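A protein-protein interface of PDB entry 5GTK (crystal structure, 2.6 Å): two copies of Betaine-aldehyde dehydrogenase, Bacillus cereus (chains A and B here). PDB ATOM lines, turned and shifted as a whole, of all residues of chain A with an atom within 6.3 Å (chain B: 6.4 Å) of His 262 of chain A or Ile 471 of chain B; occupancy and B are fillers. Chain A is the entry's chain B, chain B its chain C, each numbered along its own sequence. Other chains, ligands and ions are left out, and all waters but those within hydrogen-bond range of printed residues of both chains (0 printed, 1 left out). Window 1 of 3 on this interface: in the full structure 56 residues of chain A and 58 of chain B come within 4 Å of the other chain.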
ATOM      1  N   VAL A 158      15.241  16.430 -15.176  1.00  0.00           N
ATOM      2  CA  VAL A 158      14.319  15.658 -14.316  1.00  0.00           C
ATOM      3  C   VAL A 158      14.827  14.257 -14.014  1.00  0.00           C
ATOM      4  O   VAL A 158      14.597  13.774 -12.933  1.00  0.00           O
ATOM      5  CB  VAL A 158      12.870  15.644 -14.893  1.00  0.00           C
ATOM      6  CG1 VAL A 158      12.800  14.909 -16.235  1.00  0.00           C
ATOM      7  CG2 VAL A 158      11.876  15.067 -13.896  1.00  0.00           C
ATOM      8  N   ASP A 238      11.090   9.065 -14.251  1.00  0.00           N
ATOM      9  CA  ASP A 238      10.787  10.339 -13.588  1.00  0.00           C
ATOM     10  C   ASP A 238       9.685  11.193 -14.269  1.00  0.00           C
ATOM     11  O   ASP A 238       9.060  12.060 -13.640  1.00  0.00           O
ATOM     12  CB  ASP A 238      12.062  11.174 -13.470  1.00  0.00           C
ATOM     13  CG  ASP A 238      13.094  10.526 -12.579  1.00  0.00           C
ATOM     14  OD1 ASP A 238      12.818  10.427 -11.366  1.00  0.00           O
ATOM     15  OD2 ASP A 238      14.179  10.126 -13.108  1.00  0.00           O
ATOM     16  N   LYS A 239       9.477  10.951 -15.557  1.00  0.00           N
ATOM     17  CA  LYS A 239       8.641  11.789 -16.361  1.00  0.00           C
ATOM     18  C   LYS A 239       8.303  11.070 -17.664  1.00  0.00           C
ATOM     19  O   LYS A 239       9.115  10.254 -18.187  1.00  0.00           O
ATOM     20  CB  LYS A 239       9.397  13.080 -16.634  1.00  0.00           C
ATOM     21  CG  LYS A 239       8.571  14.184 -17.224  1.00  0.00           C
ATOM     22  CD  LYS A 239       8.666  14.252 -18.761  1.00  0.00           C
ATOM     23  CE  LYS A 239       7.465  15.110 -19.167  1.00  0.00           C
ATOM     24  NZ  LYS A 239       7.244  15.204 -20.593  1.00  0.00           N
ATOM     25  N   VAL A 240       7.103  11.352 -18.181  1.00  0.00           N
ATOM     26  CA  VAL A 240       6.647  10.663 -19.370  1.00  0.00           C
ATOM     27  C   VAL A 240       6.089  11.656 -20.408  1.00  0.00           C
ATOM     28  O   VAL A 240       5.460  12.665 -20.077  1.00  0.00           O
ATOM     29  CB  VAL A 240       5.719   9.459 -19.025  1.00  0.00           C
ATOM     30  CG1 VAL A 240       4.568   9.914 -18.183  1.00  0.00           C
ATOM     31  CG2 VAL A 240       5.157   8.753 -20.268  1.00  0.00           C
ATOM     32  N   ALA A 241       6.398  11.345 -21.671  1.00  0.00           N
ATOM     33  CA  ALA A 241       5.994  12.133 -22.824  1.00  0.00           C
ATOM     34  C   ALA A 241       5.420  11.191 -23.855  1.00  0.00           C
ATOM     35  O   ALA A 241       6.034  10.189 -24.211  1.00  0.00           O
ATOM     36  CB  ALA A 241       7.179  12.893 -23.406  1.00  0.00           C
ATOM     37  N   SER A 256       0.003   7.829 -14.802  1.00  0.00           N
ATOM     38  CA  SER A 256       1.008   8.772 -14.342  1.00  0.00           C
ATOM     39  C   SER A 256       0.619   9.409 -13.014  1.00  0.00           C
ATOM     40  O   SER A 256       1.496   9.779 -12.229  1.00  0.00           O
ATOM     41  CB  SER A 256       1.276   9.846 -15.401  1.00  0.00           C
ATOM     42  OG  SER A 256       1.995   9.304 -16.498  1.00  0.00           O
ATOM     43  N   ILE A 260       2.575  10.721  -9.207  1.00  0.00           N
ATOM     44  CA  ILE A 260       2.738  12.187  -9.412  1.00  0.00           C
ATOM     45  C   ILE A 260       3.856  12.492 -10.421  1.00  0.00           C
ATOM     46  O   ILE A 260       4.830  13.192 -10.151  1.00  0.00           O
ATOM     47  CB  ILE A 260       2.835  12.960  -8.067  1.00  0.00           C
ATOM     48  CG1 ILE A 260       1.547  12.749  -7.265  1.00  0.00           C
ATOM     49  CG2 ILE A 260       2.938  14.461  -8.259  1.00  0.00           C
ATOM     50  CD1 ILE A 260       1.679  11.690  -6.224  1.00  0.00           C
ATOM     51  N   LYS A 261       3.655  11.924 -11.605  1.00  0.00           N
ATOM     52  CA  LYS A 261       4.557  12.040 -12.743  1.00  0.00           C
ATOM     53  C   LYS A 261       4.024  13.108 -13.713  1.00  0.00           C
ATOM     54  O   LYS A 261       2.825  13.120 -14.064  1.00  0.00           O
ATOM     55  CB  LYS A 261       4.634  10.703 -13.446  1.00  0.00           C
ATOM     56  CG  LYS A 261       6.018  10.363 -13.945  1.00  0.00           C
ATOM     57  CD  LYS A 261       6.131   8.932 -14.416  1.00  0.00           C
ATOM     58  CE  LYS A 261       6.186   7.975 -13.241  1.00  0.00           C
ATOM     59  NZ  LYS A 261       6.583   6.636 -13.734  1.00  0.00           N
ATOM     60  N   HIS A 262       4.918  14.020 -14.087  1.00  0.00           N
ATOM     61  CA  HIS A 262       4.649  15.077 -15.056  1.00  0.00           C
ATOM     62  C   HIS A 262       4.426  14.385 -16.401  1.00  0.00           C
ATOM     63  O   HIS A 262       5.111  13.411 -16.737  1.00  0.00           O
ATOM     64  CB  HIS A 262       5.853  16.044 -15.081  1.00  0.00           C
ATOM     65  CG  HIS A 262       5.691  17.249 -15.958  1.00  0.00           C
ATOM     66  ND1 HIS A 262       5.836  17.198 -17.325  1.00  0.00           N
ATOM     67  CD2 HIS A 262       5.482  18.552 -15.657  1.00  0.00           C
ATOM     68  CE1 HIS A 262       5.688  18.403 -17.835  1.00  0.00           C
ATOM     69  NE2 HIS A 262       5.464  19.242 -16.844  1.00  0.00           N
ATOM     70  N   VAL A 263       3.426  14.857 -17.129  1.00  0.00           N
ATOM     71  CA  VAL A 263       3.032  14.307 -18.409  1.00  0.00           C
ATOM     72  C   VAL A 263       2.999  15.439 -19.429  1.00  0.00           C
ATOM     73  O   VAL A 263       2.593  16.576 -19.111  1.00  0.00           O
ATOM     74  CB  VAL A 263       1.607  13.705 -18.354  1.00  0.00           C
ATOM     75  CG1 VAL A 263       1.311  12.979 -19.645  1.00  0.00           C
ATOM     76  CG2 VAL A 263       1.431  12.737 -17.195  1.00  0.00           C
ATOM     77  N   THR A 264       3.452  15.144 -20.640  1.00  0.00           N
ATOM     78  CA  THR A 264       3.217  16.025 -21.764  1.00  0.00           C
ATOM     79  C   THR A 264       2.605  15.169 -22.828  1.00  0.00           C
ATOM     80  O   THR A 264       3.127  14.108 -23.121  1.00  0.00           O
ATOM     81  CB  THR A 264       4.447  16.879 -22.228  1.00  0.00           C
ATOM     82  OG1 THR A 264       5.585  16.093 -22.502  1.00  0.00           O
ATOM     83  CG2 THR A 264       4.849  17.813 -21.151  1.00  0.00           C
ATOM     84  N   ASP A 481      11.213  22.965 -20.930  1.00  0.00           N
ATOM     85  CA  ASP A 481      10.582  23.048 -19.629  1.00  0.00           C
ATOM     86  C   ASP A 481      10.077  21.718 -19.100  1.00  0.00           C
ATOM     87  O   ASP A 481      10.073  21.492 -17.883  1.00  0.00           O
ATOM     88  CB  ASP A 481       9.455  24.094 -19.654  1.00  0.00           C
ATOM     89  CG  ASP A 481       9.998  25.544 -19.763  1.00  0.00           C
ATOM     90  OD1 ASP A 481      11.221  25.804 -19.533  1.00  0.00           O
ATOM     91  OD2 ASP A 481       9.181  26.452 -20.043  1.00  0.00           O
ATOM     92  N   ASN A 482       9.683  20.825 -19.981  1.00  0.00           N
ATOM     93  CA  ASN A 482       9.172  19.507 -19.629  1.00  0.00           C
ATOM     94  C   ASN A 482      10.171  18.529 -19.117  1.00  0.00           C
ATOM     95  O   ASN A 482       9.831  17.597 -18.458  1.00  0.00           O
ATOM     96  CB  ASN A 482       8.490  18.870 -20.826  1.00  0.00           C
ATOM     97  CG  ASN A 482       7.379  19.691 -21.354  1.00  0.00           C
ATOM     98  OD1 ASN A 482       7.250  19.869 -22.520  1.00  0.00           O
ATOM     99  ND2 ASN A 482       6.603  20.211 -20.495  1.00  0.00           N
ATOM    100  N   TYR A 483      11.415  18.778 -19.445  1.00  0.00           N
ATOM    101  CA  TYR A 483      12.509  17.937 -19.085  1.00  0.00           C
ATOM    102  C   TYR A 483      13.346  18.478 -17.957  1.00  0.00           C
ATOM    103  O   TYR A 483      14.308  17.971 -17.560  1.00  0.00           O
ATOM    104  CB  TYR A 483      13.257  17.577 -20.357  1.00  0.00           C
ATOM    105  CG  TYR A 483      12.381  16.879 -21.330  1.00  0.00           C
ATOM    106  CD1 TYR A 483      11.817  15.681 -21.032  1.00  0.00           C
ATOM    107  CD2 TYR A 483      12.051  17.461 -22.533  1.00  0.00           C
ATOM    108  CE1 TYR A 483      11.011  15.064 -21.924  1.00  0.00           C
ATOM    109  CE2 TYR A 483      11.245  16.819 -23.411  1.00  0.00           C
ATOM    110  CZ  TYR A 483      10.745  15.607 -23.092  1.00  0.00           C
ATOM    111  OH  TYR A 483       9.959  14.966 -23.935  1.00  0.00           O
ATOM    112  N   THR A 484      12.861  19.538 -17.404  1.00  0.00           N
ATOM    113  CA  THR A 484      13.470  20.233 -16.339  1.00  0.00           C
ATOM    114  C   THR A 484      12.697  20.132 -15.038  1.00  0.00           C
ATOM    115  O   THR A 484      11.554  19.892 -15.010  1.00  0.00           O
ATOM    116  CB  THR A 484      13.660  21.686 -16.793  1.00  0.00           C
ATOM    117  OG1 THR A 484      14.835  21.763 -17.553  1.00  0.00           O
ATOM    118  CG2 THR A 484      13.782  22.665 -15.696  1.00  0.00           C
ATOM    119  N   MET B 253      -5.638  14.339 -10.431  1.00  0.00           N
ATOM    120  CA  MET B 253      -4.897  14.160 -11.659  1.00  0.00           C
ATOM    121  C   MET B 253      -5.582  13.061 -12.486  1.00  0.00           C
ATOM    122  O   MET B 253      -5.681  13.187 -13.716  1.00  0.00           O
ATOM    123  CB  MET B 253      -3.419  13.842 -11.391  1.00  0.00           C
ATOM    124  CG  MET B 253      -2.533  14.042 -12.615  1.00  0.00           C
ATOM    125  SD  MET B 253      -0.794  13.660 -12.292  1.00  0.00           S
ATOM    126  CE  MET B 253      -0.202  13.737 -13.975  1.00  0.00           C
ATOM    127  N   HIS B 262      -4.673  20.349 -17.885  1.00  0.00           N
ATOM    128  CA  HIS B 262      -3.435  20.713 -17.180  1.00  0.00           C
ATOM    129  C   HIS B 262      -3.674  20.736 -15.648  1.00  0.00           C
ATOM    130  O   HIS B 262      -4.707  21.240 -15.154  1.00  0.00           O
ATOM    131  CB  HIS B 262      -2.965  22.099 -17.676  1.00  0.00           C
ATOM    132  CG  HIS B 262      -1.569  22.454 -17.268  1.00  0.00           C
ATOM    133  ND1 HIS B 262      -1.264  22.902 -16.004  1.00  0.00           N
ATOM    134  CD2 HIS B 262      -0.402  22.439 -17.953  1.00  0.00           C
ATOM    135  CE1 HIS B 262       0.029  23.129 -15.917  1.00  0.00           C
ATOM    136  NE2 HIS B 262       0.573  22.861 -17.088  1.00  0.00           N
ATOM    137  N   VAL B 263      -2.732  20.176 -14.905  1.00  0.00           N
ATOM    138  CA  VAL B 263      -2.801  20.150 -13.459  1.00  0.00           C
ATOM    139  C   VAL B 263      -1.545  20.739 -12.894  1.00  0.00           C
ATOM    140  O   VAL B 263      -0.487  20.494 -13.418  1.00  0.00           O
ATOM    141  CB  VAL B 263      -2.972  18.723 -12.910  1.00  0.00           C
ATOM    142  CG1 VAL B 263      -3.236  18.772 -11.410  1.00  0.00           C
ATOM    143  CG2 VAL B 263      -4.164  18.028 -13.560  1.00  0.00           C
ATOM    144  N   THR B 264      -1.688  21.536 -11.836  1.00  0.00           N
ATOM    145  CA  THR B 264      -0.597  21.886 -10.932  1.00  0.00           C
ATOM    146  C   THR B 264      -0.956  21.272  -9.569  1.00  0.00           C
ATOM    147  O   THR B 264      -2.104  21.380  -9.126  1.00  0.00           O
ATOM    148  CB  THR B 264      -0.431  23.418 -10.800  1.00  0.00           C
ATOM    149  OG1 THR B 264      -0.209  23.994 -12.080  1.00  0.00           O
ATOM    150  CG2 THR B 264       0.767  23.786  -9.958  1.00  0.00           C
ATOM    151  N   LEU B 265       0.032  20.625  -8.934  1.00  0.00           N
ATOM    152  CA  LEU B 265      -0.102  19.941  -7.644  1.00  0.00           C
ATOM    153  C   LEU B 265       1.018  20.365  -6.744  1.00  0.00           C
ATOM    154  O   LEU B 265       2.166  20.246  -7.145  1.00  0.00           O
ATOM    155  CB  LEU B 265       0.025  18.429  -7.821  1.00  0.00           C
ATOM    156  CG  LEU B 265      -0.995  17.789  -8.737  1.00  0.00           C
ATOM    157  CD1 LEU B 265      -0.685  16.328  -8.947  1.00  0.00           C
ATOM    158  CD2 LEU B 265      -2.381  17.956  -8.146  1.00  0.00           C
ATOM    159  N   GLU B 266       0.677  20.865  -5.545  1.00  0.00           N
ATOM    160  CA  GLU B 266       1.636  21.030  -4.419  1.00  0.00           C
ATOM    161  C   GLU B 266       1.212  20.124  -3.273  1.00  0.00           C
ATOM    162  O   GLU B 266       0.186  20.369  -2.629  1.00  0.00           O
ATOM    163  CB  GLU B 266       1.688  22.462  -3.891  1.00  0.00           C
ATOM    164  CG  GLU B 266       2.023  23.544  -4.883  1.00  0.00           C
ATOM    165  CD  GLU B 266       3.508  23.848  -4.960  1.00  0.00           C
ATOM    166  OE1 GLU B 266       4.309  23.264  -4.190  1.00  0.00           O
ATOM    167  OE2 GLU B 266       3.860  24.675  -5.821  1.00  0.00           O
ATOM    168  N   LEU B 267       2.015  19.090  -3.013  1.00  0.00           N
ATOM    169  CA  LEU B 267       1.659  18.029  -2.051  1.00  0.00           C
ATOM    170  C   LEU B 267       2.639  18.006  -0.878  1.00  0.00           C
ATOM    171  O   LEU B 267       3.364  18.991  -0.648  1.00  0.00           O
ATOM    172  CB  LEU B 267       1.595  16.676  -2.760  1.00  0.00           C
ATOM    173  CG  LEU B 267       0.867  16.686  -4.087  1.00  0.00           C
ATOM    174  CD1 LEU B 267       1.016  15.347  -4.758  1.00  0.00           C
ATOM    175  CD2 LEU B 267      -0.598  17.026  -3.890  1.00  0.00           C
ATOM    176  N   GLY B 465       7.496  20.701  -5.587  1.00  0.00           N
ATOM    177  CA  GLY B 465       8.228  19.490  -5.408  1.00  0.00           C
ATOM    178  C   GLY B 465       8.704  18.654  -6.560  1.00  0.00           C
ATOM    179  O   GLY B 465       8.146  18.670  -7.592  1.00  0.00           O
ATOM    180  N   LYS B 467       9.680  14.685  -7.576  1.00  0.00           N
ATOM    181  CA  LYS B 467       8.960  13.460  -7.306  1.00  0.00           C
ATOM    182  C   LYS B 467       7.507  13.536  -6.881  1.00  0.00           C
ATOM    183  O   LYS B 467       6.722  14.135  -7.547  1.00  0.00           O
ATOM    184  CB  LYS B 467       9.725  12.670  -6.307  1.00  0.00           C
ATOM    185  CG  LYS B 467      11.172  12.538  -6.636  1.00  0.00           C
ATOM    186  CD  LYS B 467      11.994  12.583  -5.393  1.00  0.00           C
ATOM    187  CE  LYS B 467      13.240  11.779  -5.596  1.00  0.00           C
ATOM    188  NZ  LYS B 467      13.779  11.188  -4.364  1.00  0.00           N
ATOM    189  N   SER B 469       6.137  15.116  -4.384  1.00  0.00           N
ATOM    190  CA  SER B 469       5.840  16.331  -3.669  1.00  0.00           C
ATOM    191  C   SER B 469       5.021  17.281  -4.529  1.00  0.00           C
ATOM    192  O   SER B 469       4.479  18.191  -4.071  1.00  0.00           O
ATOM    193  CB  SER B 469       7.110  16.944  -3.160  1.00  0.00           C
ATOM    194  OG  SER B 469       7.436  16.343  -1.974  1.00  0.00           O
ATOM    195  N   GLY B 470       4.937  16.994  -5.796  1.00  0.00           N
ATOM    196  CA  GLY B 470       4.077  17.736  -6.718  1.00  0.00           C
ATOM    197  C   GLY B 470       4.463  17.726  -8.190  1.00  0.00           C
ATOM    198  O   GLY B 470       5.305  16.934  -8.649  1.00  0.00           O
ATOM    199  N   ILE B 471       3.761  18.578  -8.917  1.00  0.00           N
ATOM    200  CA  ILE B 471       4.010  18.864 -10.320  1.00  0.00           C
ATOM    201  C   ILE B 471       3.805  20.370 -10.459  1.00  0.00           C
ATOM    202  O   ILE B 471       2.783  20.895 -10.046  1.00  0.00           O
ATOM    203  CB  ILE B 471       3.039  18.112 -11.248  1.00  0.00           C
ATOM    204  CG1 ILE B 471       3.259  16.629 -11.106  1.00  0.00           C
ATOM    205  CG2 ILE B 471       3.238  18.475 -12.718  1.00  0.00           C
ATOM    206  CD1 ILE B 471       2.253  15.805 -11.887  1.00  0.00           C
ATOM    207  N   GLY B 472       4.812  21.047 -10.945  1.00  0.00           N
ATOM    208  CA  GLY B 472       4.799  22.467 -11.081  1.00  0.00           C
ATOM    209  C   GLY B 472       5.363  23.275  -9.946  1.00  0.00           C
ATOM    210  O   GLY B 472       5.694  22.784  -8.909  1.00  0.00           O
ATOM    211  N   ARG B 473       5.457  24.560 -10.184  1.00  0.00           N
ATOM    212  CA  ARG B 473       5.937  25.517  -9.228  1.00  0.00           C
ATOM    213  C   ARG B 473       4.952  26.655  -9.062  1.00  0.00           C
ATOM    214  O   ARG B 473       4.249  26.984  -9.937  1.00  0.00           O
ATOM    215  CB  ARG B 473       7.293  26.111  -9.627  1.00  0.00           C
ATOM    216  CG  ARG B 473       8.450  25.191  -9.817  1.00  0.00           C
ATOM    217  CD  ARG B 473       8.895  24.629  -8.506  1.00  0.00           C
ATOM    218  NE  ARG B 473       9.831  23.536  -8.551  1.00  0.00           N
ATOM    219  CZ  ARG B 473       9.530  22.267  -8.680  1.00  0.00           C
ATOM    220  NH1 ARG B 473       8.322  21.873  -8.912  1.00  0.00           N
ATOM    221  NH2 ARG B 473      10.464  21.394  -8.664  1.00  0.00           N
ATOM    222  N   ASN B 482       1.642  28.168 -15.574  1.00  0.00           N
ATOM    223  CA  ASN B 482       0.550  27.261 -15.337  1.00  0.00           C
ATOM    224  C   ASN B 482      -0.788  27.809 -15.747  1.00  0.00           C
ATOM    225  O   ASN B 482      -1.699  27.045 -15.914  1.00  0.00           O
ATOM    226  CB  ASN B 482       0.437  26.844 -13.873  1.00  0.00           C
ATOM    227  CG  ASN B 482       1.739  26.449 -13.249  1.00  0.00           C
ATOM    228  OD1 ASN B 482       2.015  26.821 -12.161  1.00  0.00           O
ATOM    229  ND2 ASN B 482       2.500  25.693 -13.922  1.00  0.00           N
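4 positions are printed for both chains.
The backbone carbonyl oxygen of Ile 260 of chain A sits close to the backbone carbonyl oxygen of Lys 467 of chain B, 3.4 Å away.
Among the printed residues, pairs that only touch across the chains: Lys 261 of chain A with Met 253 of chain B (3.1 Å), Ile 260 of chain A with Gly 470 of chain B (3.4 Å), Lys 261 of chain A with Ile 471 of chain B (3.5 Å), Ile 260 of chain A with Ile 471 of chain B (3.6 Å), Ile 260 of chain A with Leu 267 of chain B (3.6 Å), His 262 of chain A with Ile 471 of chain B (3.7 Å) and Val 263 of chain A with Met 253 of chain B (3.7 Å).
Of the 15 printed residues of chain A, 4 touch a printed residue of chain B.
Of the 15 printed residues of chain B, 5 touch a printed residue of chain A.
Printed residues of chain B that touch a printed residue of chain A: Met 253, Leu 267, Lys 467, Gly 470 and Ile 471.
Hydrophobic or aromatic side chains of chain B within 4 Å of the printed part of chain A: Met 253, Leu 267 and Ile 471.
His 262 of chain A touches just one residue of chain B: Ile 471.
Of chain A, only Ile 260 (3.6 Å), Lys 261 (3.5 Å) and His 262 (3.7 Å) come within 4 Å of Ile 471 of chain B.
Of the printed residues of chain A, Gly 470 of chain B touches Ile 260 (3.4 Å).
Of the printed residues of chain B, Ile 260 of chain A touches Leu 267, Lys 467, Gly 470 and Ile 471.
The nearest residue of chain B that does not touch His 262 of chain A is Met 253 of chain B (5.1 Å).
The nearest residue of chain A that does not touch Ile 471 of chain B is Val 263 of chain A (5.5 Å).
The backbone NH (N) of Val 240 of chain A sits at hydrogen-bond distance from the backbone carbonyl oxygen (O) of His 262 of chain A (3.2 Å).
N of Lys 261 of chain A lies within hydrogen-bond range of O of Ser 256 of chain A, at 3.1 Å.
The backbone carbonyl oxygen of Leu 265 of chain B lies within hydrogen-bond range of the backbone NH of Ile 471 of chain B.
The backbone NH of Leu 267 of chain B lies within hydrogen-bond range of the backbone carbonyl oxygen of Ser 469 of chain B (2.8 Å).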
